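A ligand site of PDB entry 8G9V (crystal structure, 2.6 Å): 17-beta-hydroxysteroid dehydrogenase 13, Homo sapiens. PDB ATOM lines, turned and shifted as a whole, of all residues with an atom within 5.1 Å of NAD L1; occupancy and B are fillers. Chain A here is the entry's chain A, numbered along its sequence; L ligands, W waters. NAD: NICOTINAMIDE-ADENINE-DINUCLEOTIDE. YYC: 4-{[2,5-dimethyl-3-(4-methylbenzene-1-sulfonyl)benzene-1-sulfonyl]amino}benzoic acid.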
ATOM      1  N   GLY A  44      11.963   7.271 -34.086  1.00  0.00           N
ATOM      2  CA  GLY A  44      10.813   6.944 -33.255  1.00  0.00           C
ATOM      3  C   GLY A  44       9.585   7.749 -33.628  1.00  0.00           C
ATOM      4  O   GLY A  44       8.760   8.060 -32.771  1.00  0.00           O
ATOM      5  N   GLY A  46       6.910   7.020 -35.314  1.00  0.00           N
ATOM      6  CA  GLY A  46       5.675   6.272 -35.489  1.00  0.00           C
ATOM      7  C   GLY A  46       4.661   6.393 -34.381  1.00  0.00           C
ATOM      8  O   GLY A  46       3.603   5.773 -34.452  1.00  0.00           O
ATOM      9  N   HIS A  47       4.964   7.183 -33.345  1.00  0.00           N
ATOM     10  CA  HIS A  47       4.052   7.341 -32.221  1.00  0.00           C
ATOM     11  C   HIS A  47       4.558   8.421 -31.244  1.00  0.00           C
ATOM     12  O   HIS A  47       5.711   8.850 -31.338  1.00  0.00           O
ATOM     13  CB  HIS A  47       3.905   5.996 -31.492  1.00  0.00           C
ATOM     14  CG  HIS A  47       2.719   5.929 -30.589  1.00  0.00           C
ATOM     15  ND1 HIS A  47       2.848   5.590 -29.254  1.00  0.00           N
ATOM     16  CD2 HIS A  47       1.415   6.168 -30.847  1.00  0.00           C
ATOM     17  CE1 HIS A  47       1.627   5.638 -28.759  1.00  0.00           C
ATOM     18  NE2 HIS A  47       0.734   5.954 -29.676  1.00  0.00           N
ATOM     19  N   GLY A  48       3.671   8.836 -30.333  1.00  0.00           N
ATOM     20  CA  GLY A  48       3.967   9.793 -29.263  1.00  0.00           C
ATOM     21  C   GLY A  48       4.704  11.065 -29.628  1.00  0.00           C
ATOM     22  O   GLY A  48       4.324  11.746 -30.585  1.00  0.00           O
ATOM     23  N   ILE A  49       5.759  11.394 -28.855  1.00  0.00           N
ATOM     24  CA  ILE A  49       6.557  12.594 -29.019  1.00  0.00           C
ATOM     25  C   ILE A  49       7.121  12.722 -30.427  1.00  0.00           C
ATOM     26  O   ILE A  49       7.034  13.788 -31.028  1.00  0.00           O
ATOM     27  CB  ILE A  49       7.633  12.677 -27.921  1.00  0.00           C
ATOM     28  CG1 ILE A  49       6.986  12.581 -26.516  1.00  0.00           C
ATOM     29  CG2 ILE A  49       8.477  13.957 -28.062  1.00  0.00           C
ATOM     30  CD1 ILE A  49       7.933  12.521 -25.365  1.00  0.00           C
ATOM     31  N   GLY A  50       7.647  11.639 -30.964  1.00  0.00           N
ATOM     32  CA  GLY A  50       8.224  11.643 -32.296  1.00  0.00           C
ATOM     33  C   GLY A  50       7.217  11.956 -33.373  1.00  0.00           C
ATOM     34  O   GLY A  50       7.518  12.709 -34.308  1.00  0.00           O
ATOM     35  N   TRP A  67      11.939   7.775 -39.205  1.00  0.00           N
ATOM     36  CA  TRP A  67      12.478   6.451 -38.905  1.00  0.00           C
ATOM     37  C   TRP A  67      11.724   5.825 -37.748  1.00  0.00           C
ATOM     38  O   TRP A  67      11.438   6.519 -36.790  1.00  0.00           O
ATOM     39  CB  TRP A  67      13.937   6.574 -38.485  1.00  0.00           C
ATOM     40  CG  TRP A  67      14.941   6.578 -39.593  1.00  0.00           C
ATOM     41  CD1 TRP A  67      14.729   6.843 -40.918  1.00  0.00           C
ATOM     42  CD2 TRP A  67      16.363   6.381 -39.443  1.00  0.00           C
ATOM     43  NE1 TRP A  67      15.924   6.790 -41.604  1.00  0.00           N
ATOM     44  CE2 TRP A  67      16.938   6.516 -40.717  1.00  0.00           C
ATOM     45  CE3 TRP A  67      17.184   6.089 -38.345  1.00  0.00           C
ATOM     46  CZ2 TRP A  67      18.311   6.353 -40.924  1.00  0.00           C
ATOM     47  CZ3 TRP A  67      18.546   5.944 -38.560  1.00  0.00           C
ATOM     48  CH2 TRP A  67      19.084   6.046 -39.844  1.00  0.00           C
ATOM     49  N   ASP A  68      11.462   4.506 -37.814  1.00  0.00           N
ATOM     50  CA  ASP A  68      10.820   3.755 -36.746  1.00  0.00           C
ATOM     51  C   ASP A  68      10.893   2.246 -37.030  1.00  0.00           C
ATOM     52  O   ASP A  68      10.949   1.847 -38.184  1.00  0.00           O
ATOM     53  CB  ASP A  68       9.345   4.176 -36.561  1.00  0.00           C
ATOM     54  CG  ASP A  68       8.782   3.914 -35.178  1.00  0.00           C
ATOM     55  OD1 ASP A  68       8.604   2.739 -34.818  1.00  0.00           O
ATOM     56  OD2 ASP A  68       8.520   4.879 -34.451  1.00  0.00           O
ATOM     57  N   ILE A  69      10.885   1.404 -35.986  1.00  0.00           N
ATOM     58  CA  ILE A  69      10.849  -0.057 -36.168  1.00  0.00           C
ATOM     59  C   ILE A  69       9.456  -0.524 -36.599  1.00  0.00           C
ATOM     60  O   ILE A  69       9.335  -1.538 -37.272  1.00  0.00           O
ATOM     61  CB  ILE A  69      11.266  -0.874 -34.938  1.00  0.00           C
ATOM     62  CG1 ILE A  69      10.625  -0.344 -33.672  1.00  0.00           C
ATOM     63  CG2 ILE A  69      12.746  -1.046 -34.807  1.00  0.00           C
ATOM     64  CD1 ILE A  69      10.642  -1.380 -32.567  1.00  0.00           C
ATOM     65  N   ASN A  70       8.409   0.191 -36.142  1.00  0.00           N
ATOM     66  CA  ASN A  70       7.005  -0.076 -36.393  1.00  0.00           C
ATOM     67  C   ASN A  70       6.603   0.490 -37.752  1.00  0.00           C
ATOM     68  O   ASN A  70       6.331   1.685 -37.876  1.00  0.00           O
ATOM     69  CB  ASN A  70       6.204   0.555 -35.239  1.00  0.00           C
ATOM     70  CG  ASN A  70       4.712   0.473 -35.303  1.00  0.00           C
ATOM     71  OD1 ASN A  70       4.125  -0.353 -35.998  1.00  0.00           O
ATOM     72  ND2 ASN A  70       4.050   1.362 -34.556  1.00  0.00           N
ATOM     73  N   VAL A  93      13.661   1.513 -39.798  1.00  0.00           N
ATOM     74  CA  VAL A  93      15.031   1.302 -39.354  1.00  0.00           C
ATOM     75  C   VAL A  93      15.037   1.009 -37.857  1.00  0.00           C
ATOM     76  O   VAL A  93      14.305   1.633 -37.104  1.00  0.00           O
ATOM     77  CB  VAL A  93      15.922   2.522 -39.680  1.00  0.00           C
ATOM     78  CG1 VAL A  93      17.380   2.284 -39.306  1.00  0.00           C
ATOM     79  CG2 VAL A  93      15.786   2.953 -41.132  1.00  0.00           C
ATOM     80  N   ASP A  94      15.844   0.014 -37.448  1.00  0.00           N
ATOM     81  CA  ASP A  94      16.018  -0.381 -36.051  1.00  0.00           C
ATOM     82  C   ASP A  94      17.213   0.389 -35.527  1.00  0.00           C
ATOM     83  O   ASP A  94      18.354   0.063 -35.863  1.00  0.00           O
ATOM     84  CB  ASP A  94      16.245  -1.898 -35.952  1.00  0.00           C
ATOM     85  CG  ASP A  94      16.458  -2.420 -34.525  1.00  0.00           C
ATOM     86  OD1 ASP A  94      16.419  -1.611 -33.576  1.00  0.00           O
ATOM     87  OD2 ASP A  94      16.663  -3.636 -34.371  1.00  0.00           O
ATOM     88  N   CYS A  95      16.953   1.419 -34.696  1.00  0.00           N
ATOM     89  CA  CYS A  95      17.999   2.283 -34.155  1.00  0.00           C
ATOM     90  C   CYS A  95      18.948   1.613 -33.158  1.00  0.00           C
ATOM     91  O   CYS A  95      19.924   2.230 -32.725  1.00  0.00           O
ATOM     92  CB  CYS A  95      17.389   3.545 -33.592  1.00  0.00           C
ATOM     93  SG  CYS A  95      16.504   4.535 -34.817  1.00  0.00           S
ATOM     94  N   SER A  96      18.700   0.336 -32.823  1.00  0.00           N
ATOM     95  CA  SER A  96      19.615  -0.428 -31.989  1.00  0.00           C
ATOM     96  C   SER A  96      20.787  -0.992 -32.842  1.00  0.00           C
ATOM     97  O   SER A  96      21.898  -1.155 -32.338  1.00  0.00           O
ATOM     98  CB  SER A  96      18.880  -1.559 -31.286  1.00  0.00           C
ATOM     99  OG  SER A  96      18.745  -2.729 -32.080  1.00  0.00           O
ATOM    100  N   ASN A 121      14.961  10.647 -31.024  1.00  0.00           N
ATOM    101  CA  ASN A 121      13.821  10.450 -30.155  1.00  0.00           C
ATOM    102  C   ASN A 121      13.568   9.007 -29.803  1.00  0.00           C
ATOM    103  O   ASN A 121      13.119   8.761 -28.695  1.00  0.00           O
ATOM    104  CB  ASN A 121      12.592  11.113 -30.759  1.00  0.00           C
ATOM    105  CG  ASN A 121      11.300  10.864 -30.032  1.00  0.00           C
ATOM    106  OD1 ASN A 121      11.018  11.466 -28.980  1.00  0.00           O
ATOM    107  ND2 ASN A 121      10.501   9.952 -30.583  1.00  0.00           N
ATOM    108  N   ALA A 122      13.824   8.029 -30.717  1.00  0.00           N
ATOM    109  CA  ALA A 122      13.559   6.605 -30.458  1.00  0.00           C
ATOM    110  C   ALA A 122      14.129   6.123 -29.127  1.00  0.00           C
ATOM    111  O   ALA A 122      15.252   6.484 -28.767  1.00  0.00           O
ATOM    112  CB  ALA A 122      14.087   5.742 -31.600  1.00  0.00           C
ATOM    113  N   GLY A 123      13.321   5.432 -28.367  1.00  0.00           N
ATOM    114  CA  GLY A 123      13.713   4.979 -27.044  1.00  0.00           C
ATOM    115  C   GLY A 123      12.973   3.717 -26.635  1.00  0.00           C
ATOM    116  O   GLY A 123      11.912   3.402 -27.170  1.00  0.00           O
ATOM    117  N   THR A 124      13.528   3.004 -25.661  1.00  0.00           N
ATOM    118  CA  THR A 124      12.942   1.769 -25.181  1.00  0.00           C
ATOM    119  C   THR A 124      13.067   1.622 -23.666  1.00  0.00           C
ATOM    120  O   THR A 124      13.992   2.161 -23.053  1.00  0.00           O
ATOM    121  CB  THR A 124      13.523   0.595 -25.975  1.00  0.00           C
ATOM    122  OG1 THR A 124      12.765  -0.572 -25.694  1.00  0.00           O
ATOM    123  CG2 THR A 124      14.961   0.356 -25.702  1.00  0.00           C
ATOM    124  N   VAL A 144      19.490   1.329 -28.010  1.00  0.00           N
ATOM    125  CA  VAL A 144      18.547   2.312 -28.523  1.00  0.00           C
ATOM    126  C   VAL A 144      18.703   3.693 -27.881  1.00  0.00           C
ATOM    127  O   VAL A 144      18.806   4.677 -28.602  1.00  0.00           O
ATOM    128  CB  VAL A 144      17.073   1.838 -28.421  1.00  0.00           C
ATOM    129  CG1 VAL A 144      16.116   2.788 -29.130  1.00  0.00           C
ATOM    130  CG2 VAL A 144      16.914   0.424 -28.945  1.00  0.00           C
ATOM    131  N   VAL A 171      16.887  13.368 -27.221  1.00  0.00           N
ATOM    132  CA  VAL A 171      15.678  13.243 -26.395  1.00  0.00           C
ATOM    133  C   VAL A 171      16.016  12.331 -25.211  1.00  0.00           C
ATOM    134  O   VAL A 171      16.031  11.101 -25.360  1.00  0.00           O
ATOM    135  CB  VAL A 171      14.409  12.776 -27.156  1.00  0.00           C
ATOM    136  CG1 VAL A 171      13.240  12.550 -26.207  1.00  0.00           C
ATOM    137  CG2 VAL A 171      14.014  13.796 -28.218  1.00  0.00           C
ATOM    138  N   ALA A 172      16.378  12.928 -24.072  1.00  0.00           N
ATOM    139  CA  ALA A 172      16.747  12.164 -22.894  1.00  0.00           C
ATOM    140  C   ALA A 172      15.493  12.023 -21.955  1.00  0.00           C
ATOM    141  O   ALA A 172      14.527  11.457 -22.468  1.00  0.00           O
ATOM    142  CB  ALA A 172      18.037  12.746 -22.235  1.00  0.00           C
ATOM    143  N   SER A 173      15.441  12.529 -20.685  1.00  0.00           N
ATOM    144  CA  SER A 173      14.348  12.382 -19.715  1.00  0.00           C
ATOM    145  C   SER A 173      14.790  12.980 -18.372  1.00  0.00           C
ATOM    146  O   SER A 173      15.991  13.173 -18.153  1.00  0.00           O
ATOM    147  CB  SER A 173      14.061  10.901 -19.511  1.00  0.00           C
ATOM    148  OG  SER A 173      13.113  10.654 -18.486  1.00  0.00           O
ATOM    149  N   VAL A 174      13.843  13.219 -17.429  1.00  0.00           N
ATOM    150  CA  VAL A 174      14.249  13.607 -16.045  1.00  0.00           C
ATOM    151  C   VAL A 174      15.042  12.460 -15.402  1.00  0.00           C
ATOM    152  O   VAL A 174      15.849  12.712 -14.514  1.00  0.00           O
ATOM    153  CB  VAL A 174      13.093  14.010 -15.114  1.00  0.00           C
ATOM    154  CG1 VAL A 174      12.712  15.446 -15.330  1.00  0.00           C
ATOM    155  CG2 VAL A 174      11.901  13.099 -15.289  1.00  0.00           C
ATOM    156  N   TYR A 186      17.131   1.879 -17.552  1.00  0.00           N
ATOM    157  CA  TYR A 186      16.584   2.982 -18.322  1.00  0.00           C
ATOM    158  C   TYR A 186      17.181   4.319 -17.881  1.00  0.00           C
ATOM    159  O   TYR A 186      17.581   5.130 -18.720  1.00  0.00           O
ATOM    160  CB  TYR A 186      15.059   3.011 -18.203  1.00  0.00           C
ATOM    161  CG  TYR A 186      14.438   4.194 -18.908  1.00  0.00           C
ATOM    162  CD1 TYR A 186      14.257   4.194 -20.285  1.00  0.00           C
ATOM    163  CD2 TYR A 186      14.017   5.313 -18.193  1.00  0.00           C
ATOM    164  CE1 TYR A 186      13.685   5.270 -20.930  1.00  0.00           C
ATOM    165  CE2 TYR A 186      13.456   6.399 -18.821  1.00  0.00           C
ATOM    166  CZ  TYR A 186      13.279   6.375 -20.193  1.00  0.00           C
ATOM    167  OH  TYR A 186      12.701   7.433 -20.824  1.00  0.00           O
ATOM    168  N   LYS A 190      19.595   6.870 -19.960  1.00  0.00           N
ATOM    169  CA  LYS A 190      19.187   8.280 -20.105  1.00  0.00           C
ATOM    170  C   LYS A 190      20.233   9.251 -19.524  1.00  0.00           C
ATOM    171  O   LYS A 190      20.392  10.359 -20.037  1.00  0.00           O
ATOM    172  CB  LYS A 190      17.806   8.518 -19.484  1.00  0.00           C
ATOM    173  CG  LYS A 190      16.682   7.872 -20.275  1.00  0.00           C
ATOM    174  CD  LYS A 190      16.488   8.569 -21.596  1.00  0.00           C
ATOM    175  CE  LYS A 190      15.692   7.767 -22.566  1.00  0.00           C
ATOM    176  NZ  LYS A 190      15.437   8.515 -23.825  1.00  0.00           N
ATOM    177  N   PRO A 219      11.878  15.588 -20.415  1.00  0.00           N
ATOM    178  CA  PRO A 219      10.533  15.712 -19.836  1.00  0.00           C
ATOM    179  C   PRO A 219      10.267  14.757 -18.679  1.00  0.00           C
ATOM    180  O   PRO A 219      10.965  13.753 -18.516  1.00  0.00           O
ATOM    181  CB  PRO A 219       9.598  15.409 -21.030  1.00  0.00           C
ATOM    182  CG  PRO A 219      10.479  14.846 -22.122  1.00  0.00           C
ATOM    183  CD  PRO A 219      11.862  14.670 -21.569  1.00  0.00           C
ATOM    184  N   VAL A 220       9.230  15.081 -17.876  1.00  0.00           N
ATOM    185  CA  VAL A 220       8.757  14.198 -16.799  1.00  0.00           C
ATOM    186  C   VAL A 220       7.797  13.173 -17.456  1.00  0.00           C
ATOM    187  O   VAL A 220       7.737  13.115 -18.689  1.00  0.00           O
ATOM    188  CB  VAL A 220       8.117  15.014 -15.636  1.00  0.00           C
ATOM    189  CG1 VAL A 220       9.148  15.860 -14.923  1.00  0.00           C
ATOM    190  CG2 VAL A 220       6.951  15.838 -16.136  1.00  0.00           C
ATOM    191  N   PHE A 221       7.067  12.338 -16.682  1.00  0.00           N
ATOM    192  CA  PHE A 221       6.158  11.356 -17.261  1.00  0.00           C
ATOM    193  C   PHE A 221       5.138  11.989 -18.223  1.00  0.00           C
ATOM    194  O   PHE A 221       4.388  12.876 -17.832  1.00  0.00           O
ATOM    195  CB  PHE A 221       5.459  10.552 -16.159  1.00  0.00           C
ATOM    196  CG  PHE A 221       4.495   9.534 -16.708  1.00  0.00           C
ATOM    197  CD1 PHE A 221       4.939   8.293 -17.118  1.00  0.00           C
ATOM    198  CD2 PHE A 221       3.154   9.843 -16.871  1.00  0.00           C
ATOM    199  CE1 PHE A 221       4.035   7.367 -17.637  1.00  0.00           C
ATOM    200  CE2 PHE A 221       2.264   8.931 -17.415  1.00  0.00           C
ATOM    201  CZ  PHE A 221       2.714   7.695 -17.789  1.00  0.00           C
ATOM    202  N   VAL A 222       5.134  11.526 -19.485  1.00  0.00           N
ATOM    203  CA  VAL A 222       4.231  11.932 -20.563  1.00  0.00           C
ATOM    204  C   VAL A 222       3.275  10.778 -20.837  1.00  0.00           C
ATOM    205  O   VAL A 222       3.687   9.605 -20.884  1.00  0.00           O
ATOM    206  CB  VAL A 222       5.003  12.310 -21.858  1.00  0.00           C
ATOM    207  CG1 VAL A 222       4.079  12.963 -22.874  1.00  0.00           C
ATOM    208  CG2 VAL A 222       6.194  13.204 -21.569  1.00  0.00           C
ATOM    209  N   THR A 224       2.026   8.833 -23.142  1.00  0.00           N
ATOM    210  CA  THR A 224       2.170   8.291 -24.503  1.00  0.00           C
ATOM    211  C   THR A 224       2.082   6.754 -24.592  1.00  0.00           C
ATOM    212  O   THR A 224       2.217   6.195 -25.682  1.00  0.00           O
ATOM    213  CB  THR A 224       3.493   8.726 -25.161  1.00  0.00           C
ATOM    214  OG1 THR A 224       4.600   8.100 -24.495  1.00  0.00           O
ATOM    215  CG2 THR A 224       3.677  10.219 -25.187  1.00  0.00           C
ATOM    216  N   GLY A 225       1.929   6.088 -23.454  1.00  0.00           N
ATOM    217  CA  GLY A 225       1.895   4.635 -23.430  1.00  0.00           C
ATOM    218  C   GLY A 225       3.255   3.970 -23.359  1.00  0.00           C
ATOM    219  O   GLY A 225       3.341   2.743 -23.262  1.00  0.00           O
ATOM    220  N   PHE A 226       4.341   4.778 -23.358  1.00  0.00           N
ATOM    221  CA  PHE A 226       5.737   4.344 -23.225  1.00  0.00           C
ATOM    222  C   PHE A 226       5.872   3.515 -21.925  1.00  0.00           C
ATOM    223  O   PHE A 226       6.404   2.395 -21.935  1.00  0.00           O
ATOM    224  CB  PHE A 226       6.655   5.592 -23.204  1.00  0.00           C
ATOM    225  CG  PHE A 226       8.136   5.307 -23.243  1.00  0.00           C
ATOM    226  CD1 PHE A 226       8.744   4.864 -24.398  1.00  0.00           C
ATOM    227  CD2 PHE A 226       8.926   5.496 -22.130  1.00  0.00           C
ATOM    228  CE1 PHE A 226      10.099   4.586 -24.427  1.00  0.00           C
ATOM    229  CE2 PHE A 226      10.280   5.245 -22.173  1.00  0.00           C
ATOM    230  CZ  PHE A 226      10.849   4.754 -23.309  1.00  0.00           C
ATOM    231  N   THR A 227       5.353   4.066 -20.823  1.00  0.00           N
ATOM    232  CA  THR A 227       5.243   3.393 -19.536  1.00  0.00           C
ATOM    233  C   THR A 227       3.758   3.464 -19.149  1.00  0.00           C
ATOM    234  O   THR A 227       3.093   4.437 -19.547  1.00  0.00           O
ATOM    235  CB  THR A 227       6.218   3.950 -18.466  1.00  0.00           C
ATOM    236  OG1 THR A 227       6.390   5.368 -18.590  1.00  0.00           O
ATOM    237  CG2 THR A 227       7.575   3.287 -18.534  1.00  0.00           C
HETATM  238  PA  NAD L   1       6.167   6.104 -27.622  1.00  0.00           P
HETATM  239  O1A NAD L   1       4.849   6.744 -27.817  1.00  0.00           O
HETATM  240  O2A NAD L   1       6.008   4.649 -27.183  1.00  0.00           O
HETATM  241  O5B NAD L   1       7.002   6.140 -29.014  1.00  0.00           O
HETATM  242  C5B NAD L   1       8.346   5.653 -29.135  1.00  0.00           C
HETATM  243  C4B NAD L   1       8.545   5.216 -30.560  1.00  0.00           C
HETATM  244  O4B NAD L   1       9.905   4.759 -30.733  1.00  0.00           O
HETATM  245  C3B NAD L   1       7.636   4.070 -31.023  1.00  0.00           C
HETATM  246  O3B NAD L   1       6.920   4.378 -32.216  1.00  0.00           O
HETATM  247  C2B NAD L   1       8.597   2.895 -31.220  1.00  0.00           C
HETATM  248  O2B NAD L   1       8.175   1.999 -32.232  1.00  0.00           O
HETATM  249  C1B NAD L   1       9.886   3.627 -31.571  1.00  0.00           C
HETATM  250  N9A NAD L   1      11.102   2.856 -31.343  1.00  0.00           N
HETATM  251  C8A NAD L   1      11.403   2.087 -30.249  1.00  0.00           C
HETATM  252  N7A NAD L   1      12.484   1.353 -30.379  1.00  0.00           N
HETATM  253  C5A NAD L   1      12.930   1.667 -31.651  1.00  0.00           C
HETATM  254  C6A NAD L   1      14.016   1.184 -32.419  1.00  0.00           C
HETATM  255  N6A NAD L   1      14.851   0.228 -31.992  1.00  0.00           N
HETATM  256  N1A NAD L   1      14.180   1.702 -33.659  1.00  0.00           N
HETATM  257  C2A NAD L   1      13.322   2.638 -34.088  1.00  0.00           C
HETATM  258  N3A NAD L   1      12.259   3.146 -33.467  1.00  0.00           N
HETATM  259  C4A NAD L   1      12.107   2.612 -32.250  1.00  0.00           C
HETATM  260  O3  NAD L   1       6.997   6.907 -26.525  1.00  0.00           O
HETATM  261  PN  NAD L   1       7.457   8.437 -26.316  1.00  0.00           P
HETATM  262  O1N NAD L   1       7.103   9.243 -27.510  1.00  0.00           O
HETATM  263  O2N NAD L   1       7.005   8.893 -24.986  1.00  0.00           O
HETATM  264  O5D NAD L   1       9.033   8.232 -26.232  1.00  0.00           O
HETATM  265  C5D NAD L   1       9.916   9.018 -27.053  1.00  0.00           C
HETATM  266  C4D NAD L   1      11.182   9.321 -26.284  1.00  0.00           C
HETATM  267  O4D NAD L   1      10.897  10.173 -25.154  1.00  0.00           O
HETATM  268  C3D NAD L   1      11.943   8.107 -25.743  1.00  0.00           C
HETATM  269  O3D NAD L   1      13.332   8.281 -25.971  1.00  0.00           O
HETATM  270  C2D NAD L   1      11.608   8.140 -24.250  1.00  0.00           C
HETATM  271  O2D NAD L   1      12.615   7.541 -23.464  1.00  0.00           O
HETATM  272  C1D NAD L   1      11.536   9.652 -24.030  1.00  0.00           C
HETATM  273  N1N NAD L   1      10.743  10.087 -22.777  1.00  0.00           N
HETATM  274  C2N NAD L   1       9.512   9.573 -22.609  1.00  0.00           C
HETATM  275  C3N NAD L   1       8.774   9.873 -21.485  1.00  0.00           C
HETATM  276  C7N NAD L   1       7.393   9.345 -21.276  1.00  0.00           C
HETATM  277  O7N NAD L   1       6.924   9.322 -20.123  1.00  0.00           O
HETATM  278  N7N NAD L   1       6.776   8.784 -22.314  1.00  0.00           N
HETATM  279  C4N NAD L   1       9.318  10.761 -20.560  1.00  0.00           C
HETATM  280  C5N NAD L   1      10.580  11.290 -20.758  1.00  0.00           C
HETATM  281  C6N NAD L   1      11.289  10.936 -21.873  1.00  0.00           C
HETATM  282  C4  YYC L   2      10.343  14.714  -8.063  1.00  0.00           C
HETATM  283  C7  YYC L   2       8.619  16.792  -7.506  1.00  0.00           C
HETATM  284  C6  YYC L   2       9.279  16.760  -8.717  1.00  0.00           C
HETATM  285  C13 YYC L   2      12.041  11.995 -11.769  1.00  0.00           C
HETATM  286  C16 YYC L   2       9.634  13.502 -11.628  1.00  0.00           C
HETATM  287  C26 YYC L   2       8.865   7.901 -16.404  1.00  0.00           C
HETATM  288  C1  YYC L   2       8.051  15.817  -5.247  1.00  0.00           C
HETATM  289  C2  YYC L   2       8.796  15.783  -6.564  1.00  0.00           C
HETATM  290  C3  YYC L   2       9.671  14.749  -6.865  1.00  0.00           C
HETATM  291  C5  YYC L   2      10.140  15.713  -8.993  1.00  0.00           C
HETATM  292  S8  YYC L   2      11.026  15.678 -10.529  1.00  0.00           S
HETATM  293  O9  YYC L   2      12.417  15.905 -10.239  1.00  0.00           O
HETATM  294  O10 YYC L   2      10.356  16.568 -11.444  1.00  0.00           O
HETATM  295  C11 YYC L   2      10.854  14.014 -11.157  1.00  0.00           C
HETATM  296  C12 YYC L   2      12.026  13.265 -11.214  1.00  0.00           C
HETATM  297  C14 YYC L   2      10.842  11.474 -12.237  1.00  0.00           C
HETATM  298  C15 YYC L   2       9.672  12.197 -12.166  1.00  0.00           C
HETATM  299  C17 YYC L   2       8.355  14.317 -11.583  1.00  0.00           C
HETATM  300  S18 YYC L   2       8.201  11.384 -12.744  1.00  0.00           S
HETATM  301  O19 YYC L   2       7.681  12.133 -13.850  1.00  0.00           O
HETATM  302  O20 YYC L   2       7.371  11.159 -11.595  1.00  0.00           O
HETATM  303  N21 YYC L   2       8.628   9.905 -13.298  1.00  0.00           N
HETATM  304  C22 YYC L   2       8.918   9.546 -14.645  1.00  0.00           C
HETATM  305  C23 YYC L   2       9.706  10.353 -15.454  1.00  0.00           C
HETATM  306  C24 YYC L   2      10.098   9.936 -16.704  1.00  0.00           C
HETATM  307  C25 YYC L   2       9.698   8.695 -17.193  1.00  0.00           C
HETATM  308  C27 YYC L   2       8.484   8.315 -15.141  1.00  0.00           C
HETATM  309  C28 YYC L   2      10.248   8.164 -18.474  1.00  0.00           C
HETATM  310  O29 YYC L   2       9.681   7.247 -19.081  1.00  0.00           O
HETATM  311  O30 YYC L   2      11.272   8.811 -18.941  1.00  0.00           O
HETATM  312  C31 YYC L   2      13.325  11.213 -11.880  1.00  0.00           C
HETATM  313  O   HOH W   1       8.102   8.889 -29.864  1.00  0.00           O
HETATM  314  O   HOH W   2      13.245  -1.655 -29.491  1.00  0.00           O
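The backbone carbonyl oxygen (O) of Val 93 lies close to a nitrogen (N1A) of NAD L1, at 3.4 Å. Gly 44 touches NAD L1 (CA to O4B, 3.5 Å). C of Gly 46 touches O3B of NAD L1, 3.7 Å away. Asn 70 touches NAD L1 (CB to O2B, 3.9 Å). Ser 96 touches NAD L1 (N to N6A, 3.9 Å). CB of Ala 122 touches N3A of NAD L1, at 3.7 Å. Gly 123 touches NAD L1 (O to C8A, 3.4 Å). Val 144 touches NAD L1. Val 171 touches NAD L1. O of Ala 172 touches C6N of NAD L1 (3.3 Å). OG of Ser 173 touches C5N of NAD L1, at 3.5 Å. O of Pro 219 touches C5N of NAD L1 (3.4 Å). Val 220 touches NAD L1 (O to C4N, 3.4 Å). Phe 221 touches NAD L1. Phe 226 touches NAD L1. Hydrophobic or aromatic side chains that line NAD L1: His 47, Ile 49, Ile 69, Ala 122, Val 144, Val 171, Tyr 186, Pro 219, Phe 221, Val 222 and Phe 226. Within 4 Å of NAD L1: Gly 44, Gly 46, His 47, Gly 48, Ile 49, Asp 68, Ile 69, Asn 70, Val 93, Asp 94, Cys 95, Ser 96, Asn 121, Ala 122, Gly 123, Val 144, Val 171, Ala 172, Ser 173, Tyr 186, Lys 190, Pro 219, Val 220, Phe 221, Val 222, Thr 224 and Phe 226. The nearest printed residue that does not touch NAD L1 is Gly 50 (4.2 Å).
Water W1 lies within hydrogen-bond range of O1N of NAD L1, ND2 of Asn 121, O of His 47, N of Gly 50 and O of Gly 44.
The backbone NH (N) of Val 93 lies within hydrogen-bond range of the backbone carbonyl oxygen (O) of Asp 68 (3.2 Å). The backbone NH of Gly 46 is in hydrogen-bond range of the side-chain carboxylate of Asp 68 (2.8 Å). The backbone NH of Asn 70 lies within hydrogen-bond range of the side-chain carboxylate of Asp 68. O of Gly 44 is in hydrogen-bond range of ND2 of Asn 121. OD1 of Asp 94 sits at hydrogen-bond distance from OG of Ser 96 (3.0 Å). The backbone carbonyl oxygen (O) of Ala 172 is in hydrogen-bond range of the side-chain amino group (NZ) of Lys 190 (3.4 Å). O of Pro 219 sits at hydrogen-bond distance from N of Val 174. N of Gly 44 is in hydrogen-bond range of O of Trp 67.
An oxygen (O2N) of NAD L1 is in hydrogen-bond range of the side-chain hydroxyl (OG1) of Thr 224, at 2.6 Å. O2D of NAD L1 lies within hydrogen-bond range of OH of Tyr 186. ND1 of His 47 lies within hydrogen-bond range of O1A of NAD L1, 2.7 Å away. The side-chain carboxylate (OD1) of Asp 68 lies within hydrogen-bond range of an oxygen (O2B) of NAD L1 (2.7 Å). The backbone carbonyl oxygen (O) of Asn 121 sits at hydrogen-bond distance from an oxygen (O3D) of NAD L1 (2.8 Å). O1N of NAD L1 lies within hydrogen-bond range of N of Ile 49 (2.9 Å). OD1 of Asp 94 is in hydrogen-bond range of N6A of NAD L1. The backbone NH (N) of Val 222 lies within hydrogen-bond range of an oxygen (O7N) of NAD L1 (2.9 Å). The backbone NH (N) of Cys 95 is in hydrogen-bond range of a nitrogen (N1A) of NAD L1, at 3.0 Å. NZ of Lys 190 sits at hydrogen-bond distance from O2D of NAD L1, 3.0 Å away. The backbone NH (N) of Ile 69 sits close to a nitrogen (N3A) of NAD L1. O1A of NAD L1 lies within hydrogen-bond range of N of Gly 48 (3.5 Å). The side-chain hydroxyl of Tyr 186 is in hydrogen-bond range of an oxygen (O30) of YYC L2. An oxygen (O30) of YYC L2 is in hydrogen-bond range of the side-chain hydroxyl of Ser 173 (2.6 Å). N of Phe 221 is in hydrogen-bond range of O19 of YYC L2, 2.9 Å away.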
